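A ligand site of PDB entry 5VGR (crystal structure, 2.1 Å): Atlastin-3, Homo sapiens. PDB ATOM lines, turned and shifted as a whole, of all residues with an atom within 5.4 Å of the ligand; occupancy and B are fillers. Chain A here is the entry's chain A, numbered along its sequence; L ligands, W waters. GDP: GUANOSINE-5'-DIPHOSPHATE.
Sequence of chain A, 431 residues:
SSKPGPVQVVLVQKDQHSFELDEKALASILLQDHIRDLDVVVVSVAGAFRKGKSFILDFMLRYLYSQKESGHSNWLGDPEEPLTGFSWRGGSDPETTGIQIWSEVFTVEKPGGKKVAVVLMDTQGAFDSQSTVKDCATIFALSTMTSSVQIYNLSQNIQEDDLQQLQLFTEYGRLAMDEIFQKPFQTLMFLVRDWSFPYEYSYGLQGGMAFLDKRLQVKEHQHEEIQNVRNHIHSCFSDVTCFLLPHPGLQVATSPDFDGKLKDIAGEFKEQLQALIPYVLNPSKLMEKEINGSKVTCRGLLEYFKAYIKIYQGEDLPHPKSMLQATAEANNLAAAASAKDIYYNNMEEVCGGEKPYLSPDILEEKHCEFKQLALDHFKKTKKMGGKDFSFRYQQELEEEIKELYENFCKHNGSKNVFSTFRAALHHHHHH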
ATOM      1  N   ALA A  48       5.853  36.420 -16.150  1.00  0.00           N
ATOM      2  CA  ALA A  48       7.006  37.268 -16.421  1.00  0.00           C
ATOM      3  C   ALA A  48       8.116  36.469 -17.108  1.00  0.00           C
ATOM      4  O   ALA A  48       8.187  35.246 -17.038  1.00  0.00           O
ATOM      5  CB  ALA A  48       7.538  37.892 -15.141  1.00  0.00           C
ATOM      6  N   PHE A  49       8.973  37.209 -17.813  1.00  0.00           N
ATOM      7  CA  PHE A  49      10.133  36.631 -18.478  1.00  0.00           C
ATOM      8  C   PHE A  49      11.030  35.926 -17.458  1.00  0.00           C
ATOM      9  O   PHE A  49      11.108  36.317 -16.297  1.00  0.00           O
ATOM     10  CB  PHE A  49      10.905  37.733 -19.219  1.00  0.00           C
ATOM     11  CG  PHE A  49      12.207  37.273 -19.841  1.00  0.00           C
ATOM     12  CD1 PHE A  49      12.221  36.255 -20.785  1.00  0.00           C
ATOM     13  CD2 PHE A  49      13.404  37.901 -19.523  1.00  0.00           C
ATOM     14  CE1 PHE A  49      13.422  35.852 -21.369  1.00  0.00           C
ATOM     15  CE2 PHE A  49      14.604  37.500 -20.097  1.00  0.00           C
ATOM     16  CZ  PHE A  49      14.616  36.470 -21.029  1.00  0.00           C
ATOM     17  N   ARG A  50      11.679  34.855 -17.911  1.00  0.00           N
ATOM     18  CA  ARG A  50      12.702  34.161 -17.135  1.00  0.00           C
ATOM     19  C   ARG A  50      12.147  33.522 -15.862  1.00  0.00           C
ATOM     20  O   ARG A  50      12.847  33.431 -14.845  1.00  0.00           O
ATOM     21  CB  ARG A  50      13.861  35.094 -16.802  1.00  0.00           C
ATOM     22  CG  ARG A  50      15.201  34.566 -17.207  1.00  0.00           C
ATOM     23  CD  ARG A  50      16.236  35.667 -17.293  1.00  0.00           C
ATOM     24  NE  ARG A  50      17.365  35.241 -18.107  1.00  0.00           N
ATOM     25  CZ  ARG A  50      18.533  35.854 -18.143  1.00  0.00           C
ATOM     26  NH1 ARG A  50      18.758  36.940 -17.400  1.00  0.00           N
ATOM     27  NH2 ARG A  50      19.484  35.384 -18.933  1.00  0.00           N
ATOM     28  N   LYS A  51      10.905  33.031 -15.891  1.00  0.00           N
ATOM     29  CA  LYS A  51      10.304  32.387 -14.730  1.00  0.00           C
ATOM     30  C   LYS A  51      10.059  30.888 -14.952  1.00  0.00           C
ATOM     31  O   LYS A  51       9.307  30.265 -14.194  1.00  0.00           O
ATOM     32  CB  LYS A  51       8.995  33.086 -14.355  1.00  0.00           C
ATOM     33  CG  LYS A  51       9.170  34.519 -13.868  1.00  0.00           C
ATOM     34  CD  LYS A  51       9.959  34.552 -12.567  1.00  0.00           C
ATOM     35  CE  LYS A  51      10.232  35.966 -12.105  1.00  0.00           C
ATOM     36  NZ  LYS A  51      11.200  36.004 -10.963  1.00  0.00           N
ATOM     37  N   GLY A  52      10.670  30.299 -15.992  1.00  0.00           N
ATOM     38  CA  GLY A  52      10.486  28.882 -16.238  1.00  0.00           C
ATOM     39  C   GLY A  52       9.271  28.486 -17.055  1.00  0.00           C
ATOM     40  O   GLY A  52       8.915  27.302 -17.062  1.00  0.00           O
ATOM     41  N   LYS A  53       8.614  29.446 -17.720  1.00  0.00           N
ATOM     42  CA  LYS A  53       7.434  29.108 -18.517  1.00  0.00           C
ATOM     43  C   LYS A  53       7.757  28.105 -19.620  1.00  0.00           C
ATOM     44  O   LYS A  53       7.025  27.141 -19.827  1.00  0.00           O
ATOM     45  CB  LYS A  53       6.828  30.377 -19.114  1.00  0.00           C
ATOM     46  CG  LYS A  53       6.286  31.377 -18.076  1.00  0.00           C
ATOM     47  CD  LYS A  53       5.533  32.530 -18.747  1.00  0.00           C
ATOM     48  CE  LYS A  53       6.403  33.180 -19.832  1.00  0.00           C
ATOM     49  NZ  LYS A  53       7.674  33.747 -19.268  1.00  0.00           N
ATOM     50  N   SER A  54       8.871  28.304 -20.314  1.00  0.00           N
ATOM     51  CA  SER A  54       9.180  27.449 -21.454  1.00  0.00           C
ATOM     52  C   SER A  54       9.663  26.065 -21.031  1.00  0.00           C
ATOM     53  O   SER A  54       9.522  25.115 -21.798  1.00  0.00           O
ATOM     54  CB  SER A  54      10.202  28.122 -22.367  1.00  0.00           C
ATOM     55  OG  SER A  54      11.498  28.067 -21.822  1.00  0.00           O
ATOM     56  N   PHE A  55      10.243  25.943 -19.828  1.00  0.00           N
ATOM     57  CA  PHE A  55      10.552  24.627 -19.279  1.00  0.00           C
ATOM     58  C   PHE A  55       9.292  23.786 -19.133  1.00  0.00           C
ATOM     59  O   PHE A  55       9.298  22.590 -19.456  1.00  0.00           O
ATOM     60  CB  PHE A  55      11.239  24.773 -17.919  1.00  0.00           C
ATOM     61  CG  PHE A  55      12.158  23.631 -17.582  1.00  0.00           C
ATOM     62  CD1 PHE A  55      13.129  23.220 -18.474  1.00  0.00           C
ATOM     63  CD2 PHE A  55      12.075  22.991 -16.351  1.00  0.00           C
ATOM     64  CE1 PHE A  55      14.003  22.168 -18.154  1.00  0.00           C
ATOM     65  CE2 PHE A  55      12.936  21.943 -16.022  1.00  0.00           C
ATOM     66  CZ  PHE A  55      13.901  21.539 -16.925  1.00  0.00           C
ATOM     67  N   ARG A  89      12.250  30.050 -27.043  1.00  0.00           N
ATOM     68  CA  ARG A  89      13.005  31.284 -26.844  1.00  0.00           C
ATOM     69  C   ARG A  89      14.115  31.452 -27.878  1.00  0.00           C
ATOM     70  O   ARG A  89      15.119  32.115 -27.601  1.00  0.00           O
ATOM     71  CB  ARG A  89      13.599  31.342 -25.440  1.00  0.00           C
ATOM     72  CG  ARG A  89      12.595  31.145 -24.317  1.00  0.00           C
ATOM     73  CD  ARG A  89      11.823  32.424 -24.015  1.00  0.00           C
ATOM     74  NE  ARG A  89      10.691  32.160 -23.127  1.00  0.00           N
ATOM     75  CZ  ARG A  89       9.424  32.221 -23.499  1.00  0.00           C
ATOM     76  NH1 ARG A  89       9.095  32.553 -24.745  1.00  0.00           N
ATOM     77  NH2 ARG A  89       8.471  31.951 -22.627  1.00  0.00           N
ATOM     78  N   GLN A 124       4.024  35.951 -22.801  1.00  0.00           N
ATOM     79  CA  GLN A 124       5.134  36.587 -22.100  1.00  0.00           C
ATOM     80  C   GLN A 124       4.960  38.101 -22.041  1.00  0.00           C
ATOM     81  O   GLN A 124       4.654  38.741 -23.047  1.00  0.00           O
ATOM     82  CB  GLN A 124       6.485  36.274 -22.757  1.00  0.00           C
ATOM     83  CG  GLN A 124       7.649  36.684 -21.852  1.00  0.00           C
ATOM     84  CD  GLN A 124       8.976  36.060 -22.240  1.00  0.00           C
ATOM     85  OE1 GLN A 124       9.341  34.996 -21.736  1.00  0.00           O
ATOM     86  NE2 GLN A 124       9.711  36.737 -23.110  1.00  0.00           N
ATOM     87  N   ASN A 153       1.865  31.760 -14.181  1.00  0.00           N
ATOM     88  CA  ASN A 153       3.117  31.185 -13.696  1.00  0.00           C
ATOM     89  C   ASN A 153       3.821  32.179 -12.773  1.00  0.00           C
ATOM     90  O   ASN A 153       4.235  33.269 -13.205  1.00  0.00           O
ATOM     91  CB  ASN A 153       4.011  30.799 -14.878  1.00  0.00           C
ATOM     92  CG  ASN A 153       5.289  30.080 -14.447  1.00  0.00           C
ATOM     93  OD1 ASN A 153       5.275  28.886 -14.161  1.00  0.00           O
ATOM     94  ND2 ASN A 153       6.413  30.812 -14.424  1.00  0.00           N
ATOM     95  N   ARG A 193       5.886  28.423  -8.576  1.00  0.00           N
ATOM     96  CA  ARG A 193       7.141  27.732  -8.822  1.00  0.00           C
ATOM     97  C   ARG A 193       8.045  27.801  -7.596  1.00  0.00           C
ATOM     98  O   ARG A 193       7.925  28.693  -6.753  1.00  0.00           O
ATOM     99  CB  ARG A 193       7.844  28.312 -10.061  1.00  0.00           C
ATOM    100  CG  ARG A 193       7.019  28.225 -11.363  1.00  0.00           C
ATOM    101  CD  ARG A 193       6.768  26.766 -11.816  1.00  0.00           C
ATOM    102  NE  ARG A 193       7.936  26.194 -12.482  1.00  0.00           N
ATOM    103  CZ  ARG A 193       8.234  26.337 -13.772  1.00  0.00           C
ATOM    104  NH1 ARG A 193       9.336  25.765 -14.245  1.00  0.00           N
ATOM    105  NH2 ARG A 193       7.416  27.002 -14.590  1.00  0.00           N
ATOM    106  N   ASP A 194       8.961  26.827  -7.503  1.00  0.00           N
ATOM    107  CA  ASP A 194       9.928  26.675  -6.409  1.00  0.00           C
ATOM    108  C   ASP A 194       9.294  26.878  -5.035  1.00  0.00           C
ATOM    109  O   ASP A 194       9.856  27.535  -4.156  1.00  0.00           O
ATOM    110  CB  ASP A 194      11.125  27.632  -6.567  1.00  0.00           C
ATOM    111  CG  ASP A 194      11.710  27.640  -7.979  1.00  0.00           C
ATOM    112  OD1 ASP A 194      12.205  28.686  -8.432  1.00  0.00           O
ATOM    113  OD2 ASP A 194      11.644  26.588  -8.644  1.00  0.00           O
ATOM    114  N   LEU A 245       4.525  23.694  -7.130  1.00  0.00           N
ATOM    115  CA  LEU A 245       5.530  22.875  -7.765  1.00  0.00           C
ATOM    116  C   LEU A 245       6.882  23.070  -7.071  1.00  0.00           C
ATOM    117  O   LEU A 245       7.229  24.203  -6.699  1.00  0.00           O
ATOM    118  CB  LEU A 245       5.636  23.227  -9.249  1.00  0.00           C
ATOM    119  CG  LEU A 245       6.424  22.330 -10.209  1.00  0.00           C
ATOM    120  CD1 LEU A 245       5.729  20.978 -10.325  1.00  0.00           C
ATOM    121  CD2 LEU A 245       6.537  22.992 -11.576  1.00  0.00           C
ATOM    122  N   PRO A 246       7.655  22.019  -6.865  1.00  0.00           N
ATOM    123  CA  PRO A 246       8.957  22.159  -6.193  1.00  0.00           C
ATOM    124  C   PRO A 246      10.018  22.746  -7.110  1.00  0.00           C
ATOM    125  O   PRO A 246       9.809  22.977  -8.304  1.00  0.00           O
ATOM    126  CB  PRO A 246       9.321  20.732  -5.775  1.00  0.00           C
ATOM    127  CG  PRO A 246       8.423  19.831  -6.576  1.00  0.00           C
ATOM    128  CD  PRO A 246       7.201  20.620  -6.937  1.00  0.00           C
ATOM    129  N   HIS A 247      11.173  22.988  -6.510  1.00  0.00           N
ATOM    130  CA  HIS A 247      12.340  23.484  -7.205  1.00  0.00           C
ATOM    131  C   HIS A 247      12.932  22.376  -8.081  1.00  0.00           C
ATOM    132  O   HIS A 247      13.010  21.215  -7.656  1.00  0.00           O
ATOM    133  CB  HIS A 247      13.364  23.966  -6.174  1.00  0.00           C
ATOM    134  CG  HIS A 247      14.448  24.847  -6.727  1.00  0.00           C
ATOM    135  ND1 HIS A 247      15.500  24.352  -7.459  1.00  0.00           N
ATOM    136  CD2 HIS A 247      14.655  26.180  -6.608  1.00  0.00           C
ATOM    137  CE1 HIS A 247      16.316  25.341  -7.774  1.00  0.00           C
ATOM    138  NE2 HIS A 247      15.821  26.464  -7.275  1.00  0.00           N
ATOM    139  N   PRO A 248      13.357  22.691  -9.318  1.00  0.00           N
ATOM    140  CA  PRO A 248      13.941  21.676 -10.200  1.00  0.00           C
ATOM    141  C   PRO A 248      15.378  21.312  -9.891  1.00  0.00           C
ATOM    142  O   PRO A 248      15.926  20.427 -10.564  1.00  0.00           O
ATOM    143  CB  PRO A 248      13.856  22.351 -11.574  1.00  0.00           C
ATOM    144  CG  PRO A 248      14.019  23.805 -11.254  1.00  0.00           C
ATOM    145  CD  PRO A 248      13.158  23.973 -10.011  1.00  0.00           C
ATOM    146  N   VAL A 252      19.301  23.052 -13.122  1.00  0.00           N
ATOM    147  CA  VAL A 252      18.287  23.691 -13.960  1.00  0.00           C
ATOM    148  C   VAL A 252      18.237  25.191 -13.673  1.00  0.00           C
ATOM    149  O   VAL A 252      18.200  26.003 -14.603  1.00  0.00           O
ATOM    150  CB  VAL A 252      16.900  23.043 -13.760  1.00  0.00           C
ATOM    151  CG1 VAL A 252      15.824  23.910 -14.426  1.00  0.00           C
ATOM    152  CG2 VAL A 252      16.845  21.623 -14.328  1.00  0.00           C
ATOM    153  N   ALA A 253      18.266  25.568 -12.389  1.00  0.00           N
ATOM    154  CA  ALA A 253      18.074  26.955 -11.993  1.00  0.00           C
ATOM    155  C   ALA A 253      19.150  27.878 -12.564  1.00  0.00           C
ATOM    156  O   ALA A 253      18.875  29.033 -12.890  1.00  0.00           O
ATOM    157  CB  ALA A 253      18.058  27.076 -10.470  1.00  0.00           C
ATOM    158  N   THR A 254      20.390  27.398 -12.655  1.00  0.00           N
ATOM    159  CA  THR A 254      21.510  28.242 -13.018  1.00  0.00           C
ATOM    160  C   THR A 254      21.973  28.025 -14.443  1.00  0.00           C
ATOM    161  O   THR A 254      23.007  28.579 -14.836  1.00  0.00           O
ATOM    162  CB  THR A 254      22.702  28.019 -12.069  1.00  0.00           C
ATOM    163  OG1 THR A 254      23.084  26.635 -12.085  1.00  0.00           O
ATOM    164  CG2 THR A 254      22.365  28.436 -10.636  1.00  0.00           C
ATOM    165  N   SER A 255      21.241  27.241 -15.231  1.00  0.00           N
ATOM    166  CA  SER A 255      21.729  26.968 -16.585  1.00  0.00           C
ATOM    167  C   SER A 255      20.984  27.789 -17.612  1.00  0.00           C
ATOM    168  O   SER A 255      19.754  27.899 -17.556  1.00  0.00           O
ATOM    169  CB  SER A 255      21.562  25.484 -16.909  1.00  0.00           C
ATOM    170  OG  SER A 255      21.538  25.269 -18.304  1.00  0.00           O
ATOM    171  N   PRO A 256      21.686  28.396 -18.581  1.00  0.00           N
ATOM    172  CA  PRO A 256      21.001  28.858 -19.787  1.00  0.00           C
ATOM    173  C   PRO A 256      20.881  27.682 -20.746  1.00  0.00           C
ATOM    174  O   PRO A 256      21.879  27.022 -21.063  1.00  0.00           O
ATOM    175  CB  PRO A 256      21.947  29.941 -20.329  1.00  0.00           C
ATOM    176  CG  PRO A 256      23.316  29.489 -19.873  1.00  0.00           C
ATOM    177  CD  PRO A 256      23.136  28.592 -18.658  1.00  0.00           C
ATOM    178  N   ASP A 257      19.655  27.393 -21.176  1.00  0.00           N
ATOM    179  CA  ASP A 257      19.408  26.250 -22.052  1.00  0.00           C
ATOM    180  C   ASP A 257      19.864  24.955 -21.392  1.00  0.00           C
ATOM    181  O   ASP A 257      20.944  24.438 -21.693  1.00  0.00           O
ATOM    182  CB  ASP A 257      20.102  26.458 -23.397  1.00  0.00           C
ATOM    183  CG  ASP A 257      19.546  25.557 -24.496  1.00  0.00           C
ATOM    184  OD1 ASP A 257      18.513  24.895 -24.265  1.00  0.00           O
ATOM    185  OD2 ASP A 257      20.154  25.518 -25.584  1.00  0.00           O
ATOM    186  N   PHE A 258      19.046  24.427 -20.480  1.00  0.00           N
ATOM    187  CA  PHE A 258      19.426  23.229 -19.738  1.00  0.00           C
ATOM    188  C   PHE A 258      19.502  22.029 -20.678  1.00  0.00           C
ATOM    189  O   PHE A 258      18.566  21.773 -21.434  1.00  0.00           O
ATOM    190  CB  PHE A 258      18.428  22.974 -18.615  1.00  0.00           C
ATOM    191  CG  PHE A 258      18.616  21.658 -17.916  1.00  0.00           C
ATOM    192  CD1 PHE A 258      19.631  21.502 -16.972  1.00  0.00           C
ATOM    193  CD2 PHE A 258      17.815  20.571 -18.224  1.00  0.00           C
ATOM    194  CE1 PHE A 258      19.823  20.306 -16.336  1.00  0.00           C
ATOM    195  CE2 PHE A 258      17.996  19.357 -17.564  1.00  0.00           C
ATOM    196  CZ  PHE A 258      19.016  19.227 -16.635  1.00  0.00           C
ATOM    197  N   PHE A 269      10.582  17.334  -8.113  1.00  0.00           N
ATOM    198  CA  PHE A 269      10.074  18.069  -9.273  1.00  0.00           C
ATOM    199  C   PHE A 269       9.530  17.110 -10.331  1.00  0.00           C
ATOM    200  O   PHE A 269       8.430  17.308 -10.857  1.00  0.00           O
ATOM    201  CB  PHE A 269      11.180  18.949  -9.856  1.00  0.00           C
ATOM    202  CG  PHE A 269      10.741  19.828 -11.010  1.00  0.00           C
ATOM    203  CD1 PHE A 269      10.196  21.076 -10.779  1.00  0.00           C
ATOM    204  CD2 PHE A 269      10.902  19.412 -12.324  1.00  0.00           C
ATOM    205  CE1 PHE A 269       9.823  21.897 -11.839  1.00  0.00           C
ATOM    206  CE2 PHE A 269      10.527  20.218 -13.392  1.00  0.00           C
ATOM    207  CZ  PHE A 269       9.974  21.462 -13.150  1.00  0.00           C
HETATM  208  PB  GDP L   1      10.768  31.717 -19.437  1.00  0.00           P
HETATM  209  O1B GDP L   1       9.639  32.031 -18.480  1.00  0.00           O
HETATM  210  O2B GDP L   1      10.311  30.846 -20.580  1.00  0.00           O
HETATM  211  O3B GDP L   1      11.297  33.065 -19.924  1.00  0.00           O
HETATM  212  O3A GDP L   1      11.938  31.021 -18.596  1.00  0.00           O
HETATM  213  PA  GDP L   1      12.843  29.778 -19.044  1.00  0.00           P
HETATM  214  O1A GDP L   1      12.040  28.520 -19.169  1.00  0.00           O
HETATM  215  O2A GDP L   1      13.656  30.114 -20.267  1.00  0.00           O
HETATM  216  O5' GDP L   1      13.800  29.621 -17.746  1.00  0.00           O
HETATM  217  C5' GDP L   1      14.644  30.661 -17.266  1.00  0.00           C
HETATM  218  C4' GDP L   1      15.739  30.054 -16.391  1.00  0.00           C
HETATM  219  O4' GDP L   1      15.172  29.394 -15.247  1.00  0.00           O
HETATM  220  C3' GDP L   1      16.524  28.993 -17.129  1.00  0.00           C
HETATM  221  O3' GDP L   1      17.847  29.034 -16.591  1.00  0.00           O
HETATM  222  C2' GDP L   1      15.854  27.691 -16.704  1.00  0.00           C
HETATM  223  O2' GDP L   1      16.708  26.549 -16.826  1.00  0.00           O
HETATM  224  C1' GDP L   1      15.496  28.004 -15.264  1.00  0.00           C
HETATM  225  N9  GDP L   1      14.303  27.291 -14.794  1.00  0.00           N
HETATM  226  C8  GDP L   1      13.368  26.618 -15.525  1.00  0.00           C
HETATM  227  N7  GDP L   1      12.396  26.135 -14.686  1.00  0.00           N
HETATM  228  C5  GDP L   1      12.710  26.510 -13.426  1.00  0.00           C
HETATM  229  C6  GDP L   1      12.150  26.345 -12.066  1.00  0.00           C
HETATM  230  O6  GDP L   1      11.087  25.714 -11.882  1.00  0.00           O
HETATM  231  N1  GDP L   1      12.820  26.896 -11.044  1.00  0.00           N
HETATM  232  C2  GDP L   1      13.969  27.600 -11.198  1.00  0.00           C
HETATM  233  N2  GDP L   1      14.606  28.136 -10.123  1.00  0.00           N
HETATM  234  N3  GDP L   1      14.533  27.784 -12.409  1.00  0.00           N
HETATM  235  C4  GDP L   1      13.958  27.276 -13.518  1.00  0.00           C
HETATM  236  O   HOH W   1       9.288  25.006  -9.983  1.00  0.00           O
HETATM  237  O   HOH W   2      16.508  30.357 -12.405  1.00  0.00           O
HETATM  238  O   HOH W   3      16.948  26.133 -19.429  1.00  0.00           O
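The backbone carbonyl oxygen (O) of Ser 255 is in hydrogen-bond range of an oxygen (O3') of the ligand (2.4 Å).
NZ of Lys 53 lies within salt-bridge range of O1B of the ligand (2.7 Å).
OD2 of Asp 194 is in hydrogen-bond range of N1 of the ligand.
The guanidinium group (NH1) of Arg 193 lies within hydrogen-bond range of an oxygen (O6) of the ligand, 2.9 Å away.
N of Gly 52 sits at hydrogen-bond distance from O3A of the ligand, 3.0 Å away.
An oxygen (O1B) of the ligand is in hydrogen-bond range of the backbone NH of Lys 51, 3.1 Å away.
NE of Arg 89 lies within salt-bridge range of O2B of the ligand (2.9 Å).
O1B of the ligand lies within hydrogen-bond range of N of Lys 53, 2.9 Å away.
O1A of the ligand sits at hydrogen-bond distance from OG of Ser 54 (2.7 Å).
O2B of the ligand lies within hydrogen-bond range of N of Ser 54 (2.9 Å).
O1A of the ligand sits at hydrogen-bond distance from N of Phe 55 (3.2 Å).
An oxygen (O3B) of the ligand sits close to the side-chain amide oxygen (OE1) of Gln 124 (3.3 Å).
An oxygen (O2') of the ligand lies within hydrogen-bond range of the backbone carbonyl oxygen of Val 252 (2.7 Å).
N of Arg 50 is in hydrogen-bond range of O3B of the ligand.
OE1 of Gln 124 sits close to NH2 of Arg 89, 3.3 Å away.
The backbone NH of Phe 258 lies close to the side-chain hydroxyl of Ser 255 (3.4 Å).
OD1 of Asn 153 sits at hydrogen-bond distance from NH2 of Arg 193, 2.9 Å away.
O of Gly 52 is in hydrogen-bond range of NH2 of Arg 193.
The backbone carbonyl oxygen (O) of Leu 245 lies within hydrogen-bond range of the backbone NH (N) of Asp 194.
The side-chain amino group (NZ) of Lys 53 lies within hydrogen-bond range of the backbone carbonyl oxygen (O) of Ala 48, 2.7 Å away.
The backbone carbonyl oxygen of Lys 51 is in hydrogen-bond range of the side-chain amide nitrogen of Asn 153, 3.0 Å away.
The side-chain amide oxygen of Gln 124 sits at hydrogen-bond distance from the side-chain amino group of Lys 53, at 3.2 Å.
Merely in contact with the ligand: Pro 248, Phe 49, His 247, Ala 253 and Ala 48.
Hydrophobic or aromatic side chains within 4 Å of the ligand: Phe 49, Phe 55, Pro 248, Val 252 and Ala 253.
Of the 25 residues printed, 17 come within 4 Å of the ligand.
The nearest printed residue that does not touch the ligand is Phe 269 (4.02 Å).
Water W3 lies within hydrogen-bond range of O2' of the ligand (2.6 Å), N of Phe 258 (2.9 Å) and N of Asp 257 (3.5 Å).
Water W1 lies within hydrogen-bond range of the backbone carbonyl oxygen (O) of Pro 246 (2.7 Å), an oxygen (O6) of the ligand (2.7 Å), the guanidinium group (NE) of Arg 193 (3.1 Å) and the backbone NH (N) of Asp 194 (3.1 Å).
Water W2 bridges O of Ala 253 (2.8 Å) and N3 of the ligand (3.2 Å).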
